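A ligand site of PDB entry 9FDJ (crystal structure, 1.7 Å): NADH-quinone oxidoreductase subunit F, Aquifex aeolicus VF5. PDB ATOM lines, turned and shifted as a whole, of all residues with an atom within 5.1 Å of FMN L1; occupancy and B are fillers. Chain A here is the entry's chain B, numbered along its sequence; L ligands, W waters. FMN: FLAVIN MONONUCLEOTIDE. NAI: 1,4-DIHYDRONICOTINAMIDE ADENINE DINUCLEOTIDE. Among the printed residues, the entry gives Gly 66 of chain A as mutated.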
ATOM      1  N   GLY A  65      19.137  -0.073 -28.085  1.00  0.00           N
ATOM      2  CA  GLY A  65      19.578  -0.363 -26.736  1.00  0.00           C
ATOM      3  C   GLY A  65      18.655  -1.335 -26.000  1.00  0.00           C
ATOM      4  O   GLY A  65      17.435  -1.210 -26.047  1.00  0.00           O
ATOM      5  N   GLY A  66      19.260  -2.280 -25.295  1.00  0.00           N
ATOM      6  CA  GLY A  66      18.534  -3.272 -24.518  1.00  0.00           C
ATOM      7  C   GLY A  66      18.418  -2.915 -23.038  1.00  0.00           C
ATOM      8  O   GLY A  66      17.907  -3.718 -22.270  1.00  0.00           O
ATOM      9  N   GLY A  67      18.844  -1.702 -22.648  1.00  0.00           N
ATOM     10  CA  GLY A  67      18.833  -1.323 -21.241  1.00  0.00           C
ATOM     11  C   GLY A  67      17.557  -0.567 -20.846  1.00  0.00           C
ATOM     12  O   GLY A  67      17.496  -0.041 -19.735  1.00  0.00           O
ATOM     13  N   GLY A  68      16.591  -0.474 -21.760  1.00  0.00           N
ATOM     14  CA  GLY A  68      15.268   0.038 -21.382  1.00  0.00           C
ATOM     15  C   GLY A  68      14.740   1.122 -22.316  1.00  0.00           C
ATOM     16  O   GLY A  68      13.531   1.199 -22.538  1.00  0.00           O
ATOM     17  N   ALA A  69      15.619   1.974 -22.835  1.00  0.00           N
ATOM     18  CA  ALA A  69      15.190   3.131 -23.616  1.00  0.00           C
ATOM     19  C   ALA A  69      15.104   2.845 -25.106  1.00  0.00           C
ATOM     20  O   ALA A  69      14.479   3.610 -25.852  1.00  0.00           O
ATOM     21  CB  ALA A  69      16.123   4.288 -23.320  1.00  0.00           C
ATOM     22  N   PHE A  71      17.299   3.204 -27.457  1.00  0.00           N
ATOM     23  CA  PHE A  71      17.941   4.215 -28.299  1.00  0.00           C
ATOM     24  C   PHE A  71      18.764   3.535 -29.398  1.00  0.00           C
ATOM     25  O   PHE A  71      19.463   2.559 -29.138  1.00  0.00           O
ATOM     26  CB  PHE A  71      18.838   5.139 -27.483  1.00  0.00           C
ATOM     27  CG  PHE A  71      19.247   6.374 -28.276  1.00  0.00           C
ATOM     28  CD1 PHE A  71      18.433   7.494 -28.292  1.00  0.00           C
ATOM     29  CD2 PHE A  71      20.416   6.389 -29.027  1.00  0.00           C
ATOM     30  CE1 PHE A  71      18.787   8.625 -29.036  1.00  0.00           C
ATOM     31  CE2 PHE A  71      20.775   7.511 -29.739  1.00  0.00           C
ATOM     32  CZ  PHE A  71      19.965   8.628 -29.747  1.00  0.00           C
ATOM     33  N   LYS A  76      23.999   6.495 -31.471  1.00  0.00           N
ATOM     34  CA  LYS A  76      24.737   6.823 -30.253  1.00  0.00           C
ATOM     35  C   LYS A  76      26.242   6.879 -30.528  1.00  0.00           C
ATOM     36  O   LYS A  76      26.926   7.837 -30.168  1.00  0.00           O
ATOM     37  CB  LYS A  76      24.448   5.822 -29.133  1.00  0.00           C
ATOM     38  CG  LYS A  76      24.821   6.299 -27.749  1.00  0.00           C
ATOM     39  CD  LYS A  76      24.758   5.254 -26.647  1.00  0.00           C
ATOM     40  CE  LYS A  76      23.390   4.685 -26.413  1.00  0.00           C
ATOM     41  NZ  LYS A  76      23.294   4.044 -25.093  1.00  0.00           N
ATOM     42  N   ASN A  92      27.203  -1.655 -19.385  1.00  0.00           N
ATOM     43  CA  ASN A  92      26.325  -1.579 -18.232  1.00  0.00           C
ATOM     44  C   ASN A  92      25.736  -2.957 -17.917  1.00  0.00           C
ATOM     45  O   ASN A  92      24.821  -3.386 -18.596  1.00  0.00           O
ATOM     46  CB  ASN A  92      25.209  -0.596 -18.522  1.00  0.00           C
ATOM     47  CG  ASN A  92      24.400  -0.233 -17.294  1.00  0.00           C
ATOM     48  OD1 ASN A  92      24.417  -0.955 -16.289  1.00  0.00           O
ATOM     49  ND2 ASN A  92      23.758   0.913 -17.361  1.00  0.00           N
ATOM     50  N   ASP A  94      24.605  -3.528 -14.673  1.00  0.00           N
ATOM     51  CA  ASP A  94      24.051  -3.260 -13.364  1.00  0.00           C
ATOM     52  C   ASP A  94      22.736  -3.985 -13.102  1.00  0.00           C
ATOM     53  O   ASP A  94      22.372  -4.093 -11.931  1.00  0.00           O
ATOM     54  CB  ASP A  94      23.854  -1.784 -13.062  1.00  0.00           C
ATOM     55  CG  ASP A  94      23.782  -1.531 -11.560  1.00  0.00           C
ATOM     56  OD1 ASP A  94      24.780  -1.898 -10.887  1.00  0.00           O
ATOM     57  OD2 ASP A  94      22.689  -1.132 -11.067  1.00  0.00           O
ATOM     58  N   GLU A  95      22.025  -4.389 -14.169  1.00  0.00           N
ATOM     59  CA  GLU A  95      20.752  -5.109 -14.142  1.00  0.00           C
ATOM     60  C   GLU A  95      20.163  -5.333 -12.748  1.00  0.00           C
ATOM     61  O   GLU A  95      20.405  -6.361 -12.103  1.00  0.00           O
ATOM     62  CB  GLU A  95      20.942  -6.452 -14.843  1.00  0.00           C
ATOM     63  CG  GLU A  95      19.682  -7.288 -14.898  1.00  0.00           C
ATOM     64  CD  GLU A  95      19.795  -8.450 -15.847  1.00  0.00           C
ATOM     65  OE1 GLU A  95      20.510  -9.423 -15.478  1.00  0.00           O
ATOM     66  OE2 GLU A  95      19.170  -8.360 -16.926  1.00  0.00           O
ATOM     67  N   SER A  96      19.340  -4.378 -12.294  1.00  0.00           N
ATOM     68  CA  SER A  96      18.750  -4.453 -10.966  1.00  0.00           C
ATOM     69  C   SER A  96      17.261  -4.115 -10.945  1.00  0.00           C
ATOM     70  O   SER A  96      16.678  -3.990  -9.873  1.00  0.00           O
ATOM     71  CB  SER A  96      19.520  -3.537 -10.017  1.00  0.00           C
ATOM     72  OG  SER A  96      20.817  -4.064  -9.771  1.00  0.00           O
ATOM     73  N   ASP A 103      20.396 -10.162 -18.624  1.00  0.00           N
ATOM     74  CA  ASP A 103      21.795  -9.883 -18.936  1.00  0.00           C
ATOM     75  C   ASP A 103      22.730 -10.882 -18.244  1.00  0.00           C
ATOM     76  O   ASP A 103      23.773 -11.254 -18.795  1.00  0.00           O
ATOM     77  CB  ASP A 103      22.175  -8.466 -18.515  1.00  0.00           C
ATOM     78  CG  ASP A 103      21.437  -7.334 -19.218  1.00  0.00           C
ATOM     79  OD1 ASP A 103      20.888  -7.570 -20.307  1.00  0.00           O
ATOM     80  OD2 ASP A 103      21.437  -6.228 -18.636  1.00  0.00           O
ATOM     81  N   TYR A 180      20.527   0.478  -7.096  1.00  0.00           N
ATOM     82  CA  TYR A 180      19.844   0.397  -8.368  1.00  0.00           C
ATOM     83  C   TYR A 180      20.180   1.596  -9.248  1.00  0.00           C
ATOM     84  O   TYR A 180      20.281   1.460 -10.460  1.00  0.00           O
ATOM     85  CB  TYR A 180      18.336   0.324  -8.192  1.00  0.00           C
ATOM     86  CG  TYR A 180      17.480   0.561  -9.434  1.00  0.00           C
ATOM     87  CD1 TYR A 180      17.465  -0.345 -10.492  1.00  0.00           C
ATOM     88  CD2 TYR A 180      16.639   1.661  -9.521  1.00  0.00           C
ATOM     89  CE1 TYR A 180      16.651  -0.150 -11.587  1.00  0.00           C
ATOM     90  CE2 TYR A 180      15.817   1.868 -10.618  1.00  0.00           C
ATOM     91  CZ  TYR A 180      15.837   0.951 -11.666  1.00  0.00           C
ATOM     92  OH  TYR A 180      15.066   1.146 -12.777  1.00  0.00           O
ATOM     93  N   ILE A 181      20.335   2.774  -8.628  1.00  0.00           N
ATOM     94  CA  ILE A 181      20.529   3.993  -9.403  1.00  0.00           C
ATOM     95  C   ILE A 181      21.852   3.970 -10.159  1.00  0.00           C
ATOM     96  O   ILE A 181      21.995   4.691 -11.129  1.00  0.00           O
ATOM     97  CB  ILE A 181      20.400   5.224  -8.486  1.00  0.00           C
ATOM     98  CG1 ILE A 181      20.260   6.516  -9.260  1.00  0.00           C
ATOM     99  CG2 ILE A 181      21.571   5.254  -7.515  1.00  0.00           C
ATOM    100  CD1 ILE A 181      19.131   6.526 -10.252  1.00  0.00           C
ATOM    101  N   GLY A 183      22.694   1.872 -12.210  1.00  0.00           N
ATOM    102  CA  GLY A 183      22.401   1.474 -13.580  1.00  0.00           C
ATOM    103  C   GLY A 183      22.095   2.660 -14.507  1.00  0.00           C
ATOM    104  O   GLY A 183      22.124   2.535 -15.730  1.00  0.00           O
ATOM    105  N   GLU A 184      21.744   3.814 -13.913  1.00  0.00           N
ATOM    106  CA  GLU A 184      21.542   5.024 -14.688  1.00  0.00           C
ATOM    107  C   GLU A 184      22.922   5.457 -15.169  1.00  0.00           C
ATOM    108  O   GLU A 184      23.839   5.527 -14.361  1.00  0.00           O
ATOM    109  CB  GLU A 184      20.835   6.092 -13.847  1.00  0.00           C
ATOM    110  CG  GLU A 184      20.246   7.234 -14.658  1.00  0.00           C
ATOM    111  CD  GLU A 184      21.216   8.320 -15.092  1.00  0.00           C
ATOM    112  OE1 GLU A 184      22.304   8.465 -14.491  1.00  0.00           O
ATOM    113  OE2 GLU A 184      20.857   9.072 -16.023  1.00  0.00           O
ATOM    114  N   GLU A 185      23.074   5.679 -16.467  1.00  0.00           N
ATOM    115  CA  GLU A 185      24.396   5.747 -17.084  1.00  0.00           C
ATOM    116  C   GLU A 185      25.286   6.839 -16.453  1.00  0.00           C
ATOM    117  O   GLU A 185      26.494   6.650 -16.340  1.00  0.00           O
ATOM    118  CB  GLU A 185      24.246   5.937 -18.590  1.00  0.00           C
ATOM    119  CG  GLU A 185      23.571   7.240 -18.958  1.00  0.00           C
ATOM    120  CD  GLU A 185      23.387   7.435 -20.451  1.00  0.00           C
ATOM    121  OE1 GLU A 185      23.882   6.596 -21.242  1.00  0.00           O
ATOM    122  OE2 GLU A 185      22.762   8.463 -20.786  1.00  0.00           O
ATOM    123  N   LYS A 202      21.424  15.855 -17.592  1.00  0.00           N
ATOM    124  CA  LYS A 202      21.620  15.568 -19.011  1.00  0.00           C
ATOM    125  C   LYS A 202      20.677  16.478 -19.795  1.00  0.00           C
ATOM    126  O   LYS A 202      19.564  16.720 -19.342  1.00  0.00           O
ATOM    127  CB  LYS A 202      21.244  14.116 -19.347  1.00  0.00           C
ATOM    128  CG  LYS A 202      22.061  13.028 -18.688  1.00  0.00           C
ATOM    129  CD  LYS A 202      21.323  11.703 -18.493  1.00  0.00           C
ATOM    130  CE  LYS A 202      20.882  10.930 -19.708  1.00  0.00           C
ATOM    131  NZ  LYS A 202      20.532   9.520 -19.386  1.00  0.00           N
ATOM    132  N   VAL A 218      27.921   4.413 -23.192  1.00  0.00           N
ATOM    133  CA  VAL A 218      27.415   3.409 -22.268  1.00  0.00           C
ATOM    134  C   VAL A 218      26.405   2.570 -23.055  1.00  0.00           C
ATOM    135  O   VAL A 218      25.485   3.134 -23.667  1.00  0.00           O
ATOM    136  CB  VAL A 218      26.775   4.020 -21.012  1.00  0.00           C
ATOM    137  CG1 VAL A 218      26.230   2.968 -20.074  1.00  0.00           C
ATOM    138  CG2 VAL A 218      27.733   4.935 -20.282  1.00  0.00           C
ATOM    139  N   ASN A 219      26.600   1.254 -23.051  1.00  0.00           N
ATOM    140  CA  ASN A 219      25.631   0.347 -23.639  1.00  0.00           C
ATOM    141  C   ASN A 219      25.386  -0.826 -22.703  1.00  0.00           C
ATOM    142  O   ASN A 219      26.250  -1.267 -21.951  1.00  0.00           O
ATOM    143  CB  ASN A 219      26.038  -0.229 -25.008  1.00  0.00           C
ATOM    144  CG  ASN A 219      25.681   0.665 -26.169  1.00  0.00           C
ATOM    145  OD1 ASN A 219      24.516   1.064 -26.360  1.00  0.00           O
ATOM    146  ND2 ASN A 219      26.706   1.050 -26.895  1.00  0.00           N
ATOM    147  N   ASN A 220      24.175  -1.342 -22.809  1.00  0.00           N
ATOM    148  CA  ASN A 220      23.716  -2.485 -22.041  1.00  0.00           C
ATOM    149  C   ASN A 220      24.353  -3.781 -22.546  1.00  0.00           C
ATOM    150  O   ASN A 220      24.671  -3.889 -23.719  1.00  0.00           O
ATOM    151  CB  ASN A 220      22.191  -2.529 -22.126  1.00  0.00           C
ATOM    152  CG  ASN A 220      21.600  -3.717 -21.423  1.00  0.00           C
ATOM    153  OD1 ASN A 220      21.534  -3.792 -20.186  1.00  0.00           O
ATOM    154  ND2 ASN A 220      21.193  -4.679 -22.221  1.00  0.00           N
ATOM    155  N   VAL A 221      24.501  -4.748 -21.637  1.00  0.00           N
ATOM    156  CA  VAL A 221      25.036  -6.077 -21.945  1.00  0.00           C
ATOM    157  C   VAL A 221      24.388  -6.651 -23.207  1.00  0.00           C
ATOM    158  O   VAL A 221      25.112  -7.069 -24.131  1.00  0.00           O
ATOM    159  CB  VAL A 221      24.842  -7.032 -20.761  1.00  0.00           C
ATOM    160  CG1 VAL A 221      25.056  -8.501 -21.136  1.00  0.00           C
ATOM    161  CG2 VAL A 221      25.733  -6.627 -19.566  1.00  0.00           C
ATOM    162  N   THR A 223      22.703  -5.205 -25.667  1.00  0.00           N
ATOM    163  CA  THR A 223      23.034  -4.441 -26.846  1.00  0.00           C
ATOM    164  C   THR A 223      24.376  -4.904 -27.423  1.00  0.00           C
ATOM    165  O   THR A 223      24.516  -5.140 -28.620  1.00  0.00           O
ATOM    166  CB  THR A 223      23.072  -2.952 -26.512  1.00  0.00           C
ATOM    167  OG1 THR A 223      21.942  -2.618 -25.699  1.00  0.00           O
ATOM    168  CG2 THR A 223      23.153  -2.126 -27.779  1.00  0.00           C
ATOM    169  N   CYS A 393      16.659  12.503 -13.403  1.00  0.00           N
ATOM    170  CA  CYS A 393      16.867  11.222 -14.058  1.00  0.00           C
ATOM    171  C   CYS A 393      15.538  10.468 -14.168  1.00  0.00           C
ATOM    172  O   CYS A 393      14.532  10.896 -13.625  1.00  0.00           O
ATOM    173  CB  CYS A 393      17.956  10.398 -13.366  1.00  0.00           C
ATOM    174  SG  CYS A 393      17.361   9.263 -12.069  1.00  0.00           S
ATOM    175  N   GLY A 394      15.557   9.338 -14.866  1.00  0.00           N
ATOM    176  CA  GLY A 394      14.332   8.605 -15.154  1.00  0.00           C
ATOM    177  C   GLY A 394      13.634   7.993 -13.939  1.00  0.00           C
ATOM    178  O   GLY A 394      12.448   7.712 -14.007  1.00  0.00           O
ATOM    179  N   LEU A 395      14.355   7.758 -12.828  1.00  0.00           N
ATOM    180  CA  LEU A 395      13.737   7.121 -11.667  1.00  0.00           C
ATOM    181  C   LEU A 395      12.595   7.990 -11.160  1.00  0.00           C
ATOM    182  O   LEU A 395      11.482   7.519 -10.969  1.00  0.00           O
ATOM    183  CB  LEU A 395      14.772   6.827 -10.587  1.00  0.00           C
ATOM    184  CG  LEU A 395      14.284   5.953  -9.412  1.00  0.00           C
ATOM    185  CD1 LEU A 395      15.408   5.210  -8.729  1.00  0.00           C
ATOM    186  CD2 LEU A 395      13.557   6.818  -8.387  1.00  0.00           C
HETATM  187  N1  FMN L   1      20.634   0.433 -18.338  1.00  0.00           N
HETATM  188  C2  FMN L   1      21.278  -0.795 -18.263  1.00  0.00           C
HETATM  189  O2  FMN L   1      21.951  -1.236 -19.230  1.00  0.00           O
HETATM  190  N3  FMN L   1      21.221  -1.511 -17.087  1.00  0.00           N
HETATM  191  C4  FMN L   1      20.585  -1.106 -15.914  1.00  0.00           C
HETATM  192  O4  FMN L   1      20.659  -1.799 -14.906  1.00  0.00           O
HETATM  193  C4A FMN L   1      19.920   0.191 -16.005  1.00  0.00           C
HETATM  194  N5  FMN L   1      19.339   0.676 -14.920  1.00  0.00           N
HETATM  195  C5A FMN L   1      18.809   1.967 -15.014  1.00  0.00           C
HETATM  196  C6  FMN L   1      18.244   2.550 -13.863  1.00  0.00           C
HETATM  197  C7  FMN L   1      17.687   3.813 -13.913  1.00  0.00           C
HETATM  198  C7M FMN L   1      17.056   4.388 -12.656  1.00  0.00           C
HETATM  199  C8  FMN L   1      17.658   4.527 -15.124  1.00  0.00           C
HETATM  200  C8M FMN L   1      16.925   5.849 -15.261  1.00  0.00           C
HETATM  201  C9  FMN L   1      18.240   3.966 -16.262  1.00  0.00           C
HETATM  202  C9A FMN L   1      18.813   2.696 -16.213  1.00  0.00           C
HETATM  203  N10 FMN L   1      19.410   2.111 -17.348  1.00  0.00           N
HETATM  204  C10 FMN L   1      19.995   0.873 -17.250  1.00  0.00           C
HETATM  205  C1' FMN L   1      19.473   2.813 -18.626  1.00  0.00           C
HETATM  206  C2' FMN L   1      20.829   3.491 -18.822  1.00  0.00           C
HETATM  207  O2' FMN L   1      20.831   4.797 -18.217  1.00  0.00           O
HETATM  208  C3' FMN L   1      21.209   3.599 -20.305  1.00  0.00           C
HETATM  209  O3' FMN L   1      20.122   4.098 -21.074  1.00  0.00           O
HETATM  210  C4' FMN L   1      21.670   2.303 -20.955  1.00  0.00           C
HETATM  211  O4' FMN L   1      22.665   1.650 -20.151  1.00  0.00           O
HETATM  212  C5' FMN L   1      22.209   2.625 -22.330  1.00  0.00           C
HETATM  213  O5' FMN L   1      22.562   1.414 -23.072  1.00  0.00           O
HETATM  214  P   FMN L   1      21.631   0.927 -24.243  1.00  0.00           P
HETATM  215  O1P FMN L   1      22.442  -0.230 -24.846  1.00  0.00           O
HETATM  216  O2P FMN L   1      21.368   2.043 -25.195  1.00  0.00           O
HETATM  217  O3P FMN L   1      20.306   0.499 -23.639  1.00  0.00           O
HETATM  218  PA  NAI L   2      17.248   8.001 -22.375  1.00  0.00           P
HETATM  219  O1A NAI L   2      16.032   7.931 -23.206  1.00  0.00           O
HETATM  220  O2A NAI L   2      17.564   9.432 -21.878  1.00  0.00           O
HETATM  221  O5B NAI L   2      18.577   7.617 -23.191  1.00  0.00           O
HETATM  222  C5B NAI L   2      18.819   6.240 -23.577  1.00  0.00           C
HETATM  223  C4B NAI L   2      20.216   6.181 -24.126  1.00  0.00           C
HETATM  224  O4B NAI L   2      20.285   7.024 -25.298  1.00  0.00           O
HETATM  225  C3B NAI L   2      21.282   6.720 -23.164  1.00  0.00           C
HETATM  226  O3B NAI L   2      22.541   6.064 -23.352  1.00  0.00           O
HETATM  227  C2B NAI L   2      21.396   8.185 -23.575  1.00  0.00           C
HETATM  228  O2B NAI L   2      22.663   8.748 -23.245  1.00  0.00           O
HETATM  229  C1B NAI L   2      21.231   8.071 -25.107  1.00  0.00           C
HETATM  230  N9A NAI L   2      20.715   9.267 -25.769  1.00  0.00           N
HETATM  231  C8A NAI L   2      19.392   9.664 -25.830  1.00  0.00           C
HETATM  232  N7A NAI L   2      19.202  10.770 -26.508  1.00  0.00           N
HETATM  233  C5A NAI L   2      20.479  11.132 -26.918  1.00  0.00           C
HETATM  234  C6A NAI L   2      20.968  12.235 -27.635  1.00  0.00           C
HETATM  235  N6A NAI L   2      20.193  13.196 -28.153  1.00  0.00           N
HETATM  236  N1A NAI L   2      22.305  12.325 -27.819  1.00  0.00           N
HETATM  237  C2A NAI L   2      23.094  11.370 -27.321  1.00  0.00           C
HETATM  238  N3A NAI L   2      22.747  10.266 -26.647  1.00  0.00           N
HETATM  239  C4A NAI L   2      21.425  10.210 -26.469  1.00  0.00           C
HETATM  240  O3  NAI L   2      17.150   6.958 -21.169  1.00  0.00           O
HETATM  241  PN  NAI L   2      17.751   6.668 -19.718  1.00  0.00           P
HETATM  242  O1N NAI L   2      17.375   7.890 -18.824  1.00  0.00           O
HETATM  243  O2N NAI L   2      19.182   6.388 -19.736  1.00  0.00           O
HETATM  244  O5D NAI L   2      16.878   5.327 -19.258  1.00  0.00           O
HETATM  245  C5D NAI L   2      15.463   5.078 -19.012  1.00  0.00           C
HETATM  246  O   HOH W   1      18.947   3.041 -25.151  1.00  0.00           O
HETATM  247  O   HOH W   2      20.243  -0.818 -12.183  1.00  0.00           O
HETATM  248  O   HOH W   3      15.167   2.438 -16.227  1.00  0.00           O
HETATM  249  O   HOH W   4      17.206  -1.217 -17.002  1.00  0.00           O
HETATM  250  O   HOH W   5      21.815   1.894 -27.877  1.00  0.00           O
HETATM  251  O   HOH W   6      22.556  -4.208 -17.183  1.00  0.00           O
HETATM  252  O   HOH W   7      18.538   2.046 -22.454  1.00  0.00           O
HETATM  253  O   HOH W   8      15.894   0.151 -15.233  1.00  0.00           O
HETATM  254  O   HOH W   9      18.081  -2.789 -14.468  1.00  0.00           O
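An oxygen (O1P) of FMN L1 lies close to the side-chain amide oxygen (OD1) of Asn 219 (2.9 Å).
The side-chain carboxylate (OE2) of Glu 185 is in hydrogen-bond range of an oxygen (O2B) of NAI L2 (2.5 Å).
O2P of FMN L1 is in salt-bridge range of NZ of Lys 76.
The side-chain amino group (NZ) of Lys 202 lies within salt-bridge range of an oxygen (O2N) of NAI L2 (3.4 Å).
An oxygen (O4') of FMN L1 is in hydrogen-bond range of the side-chain amide nitrogen (ND2) of Asn 92.
An oxygen (O3P) of FMN L1 sits at hydrogen-bond distance from the backbone NH (N) of Gly 66, 3.4 Å away.
OG1 of Thr 223 lies within hydrogen-bond range of O1P of FMN L1.
An oxygen (O2) of FMN L1 lies close to the side-chain amide oxygen of Asn 220 (2.8 Å).
The backbone NH (N) of Glu 95 sits at hydrogen-bond distance from an oxygen (O4) of FMN L1 (3.0 Å).
The side-chain amino group of Lys 76 lies within hydrogen-bond range of an oxygen (O3B) of NAI L2, at 2.8 Å.
An oxygen (O3P) of FMN L1 is in hydrogen-bond range of the backbone NH of Gly 67.
O2' of FMN L1 lies within hydrogen-bond range of N of Glu 185, 3.0 Å away.
The backbone NH of Asn 220 is in hydrogen-bond range of an oxygen (O1P) of FMN L1.
An oxygen (O2') of FMN L1 lies within hydrogen-bond range of an oxygen (O2N) of NAI L2 (2.7 Å).
The backbone NH (N) of Gly 183 lies within hydrogen-bond range of the side-chain carboxylate (OD2) of Asp 94, 3.2 Å away.
The backbone NH of Gly 65 lies within hydrogen-bond range of the backbone carbonyl oxygen of Phe 71, at 2.9 Å.
The backbone carbonyl oxygen (O) of Gly 66 lies close to the side-chain amide nitrogen (ND2) of Asn 220 (3.4 Å).
O of Asp 94 lies within hydrogen-bond range of OG of Ser 96.
The side-chain amino group (NZ) of Lys 202 is in salt-bridge range of the side-chain carboxylate (OE2) of Glu 185, at 2.8 Å.
The side-chain amino group (NZ) of Lys 202 lies within salt-bridge range of the side-chain carboxylate (OE2) of Glu 184, at 3.4 Å.
The side-chain amide oxygen (OD1) of Asn 219 lies within hydrogen-bond range of the side-chain amino group (NZ) of Lys 76, 3.5 Å away.
The backbone NH (N) of Asp 94 lies within hydrogen-bond range of the side-chain amide oxygen (OD1) of Asn 92 (3.0 Å).
O of Gly 183 lies close to N10 of FMN L1 (3.2 Å).
An oxygen (O5') of FMN L1 lies close to the backbone carbonyl oxygen (O) of Val 218, at 3.4 Å.
Merely in contact with FMN L1: Gly 65, Asp 94, Ser 96, Tyr 180, Ile 181, Glu 184, Gly 394 and Leu 395.
Hydrophobic or aromatic side chains that line FMN L1: Tyr 180, Ile 181, Val 218 and Leu 395.
Within 4 Å of FMN L1: Gly 65, Gly 66, Gly 67, Lys 76, Asn 92, Asp 94, Glu 95, Ser 96, Tyr 180, Ile 181, Gly 183, Glu 184, Glu 185, Val 218, Asn 219, Asn 220, Thr 223, Gly 394 and Leu 395.
The nearest printed residue that does not touch FMN L1 is Gly 68 (4.3 Å).
Water W1 lies within hydrogen-bond range of an oxygen (O2P) of FMN L1 and the backbone NH (N) of Phe 71.
Water W7 lies within hydrogen-bond range of an oxygen (O3P) of FMN L1 (2.6 Å), the backbone NH (N) of Ala 69 (2.9 Å) and the backbone NH (N) of Gly 68 (3.3 Å).
Water W5 lies within hydrogen-bond range of O2P of FMN L1, O of Phe 71, OD1 of Asn 219 and N of Gly 65.
Water W9 lies within hydrogen-bond range of an oxygen (O4) of FMN L1 (2.8 Å) and the backbone NH (N) of Ser 96 (3.0 Å).
Water W8 bridges the side-chain hydroxyl of Tyr 180 and a nitrogen (N5) of FMN L1.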
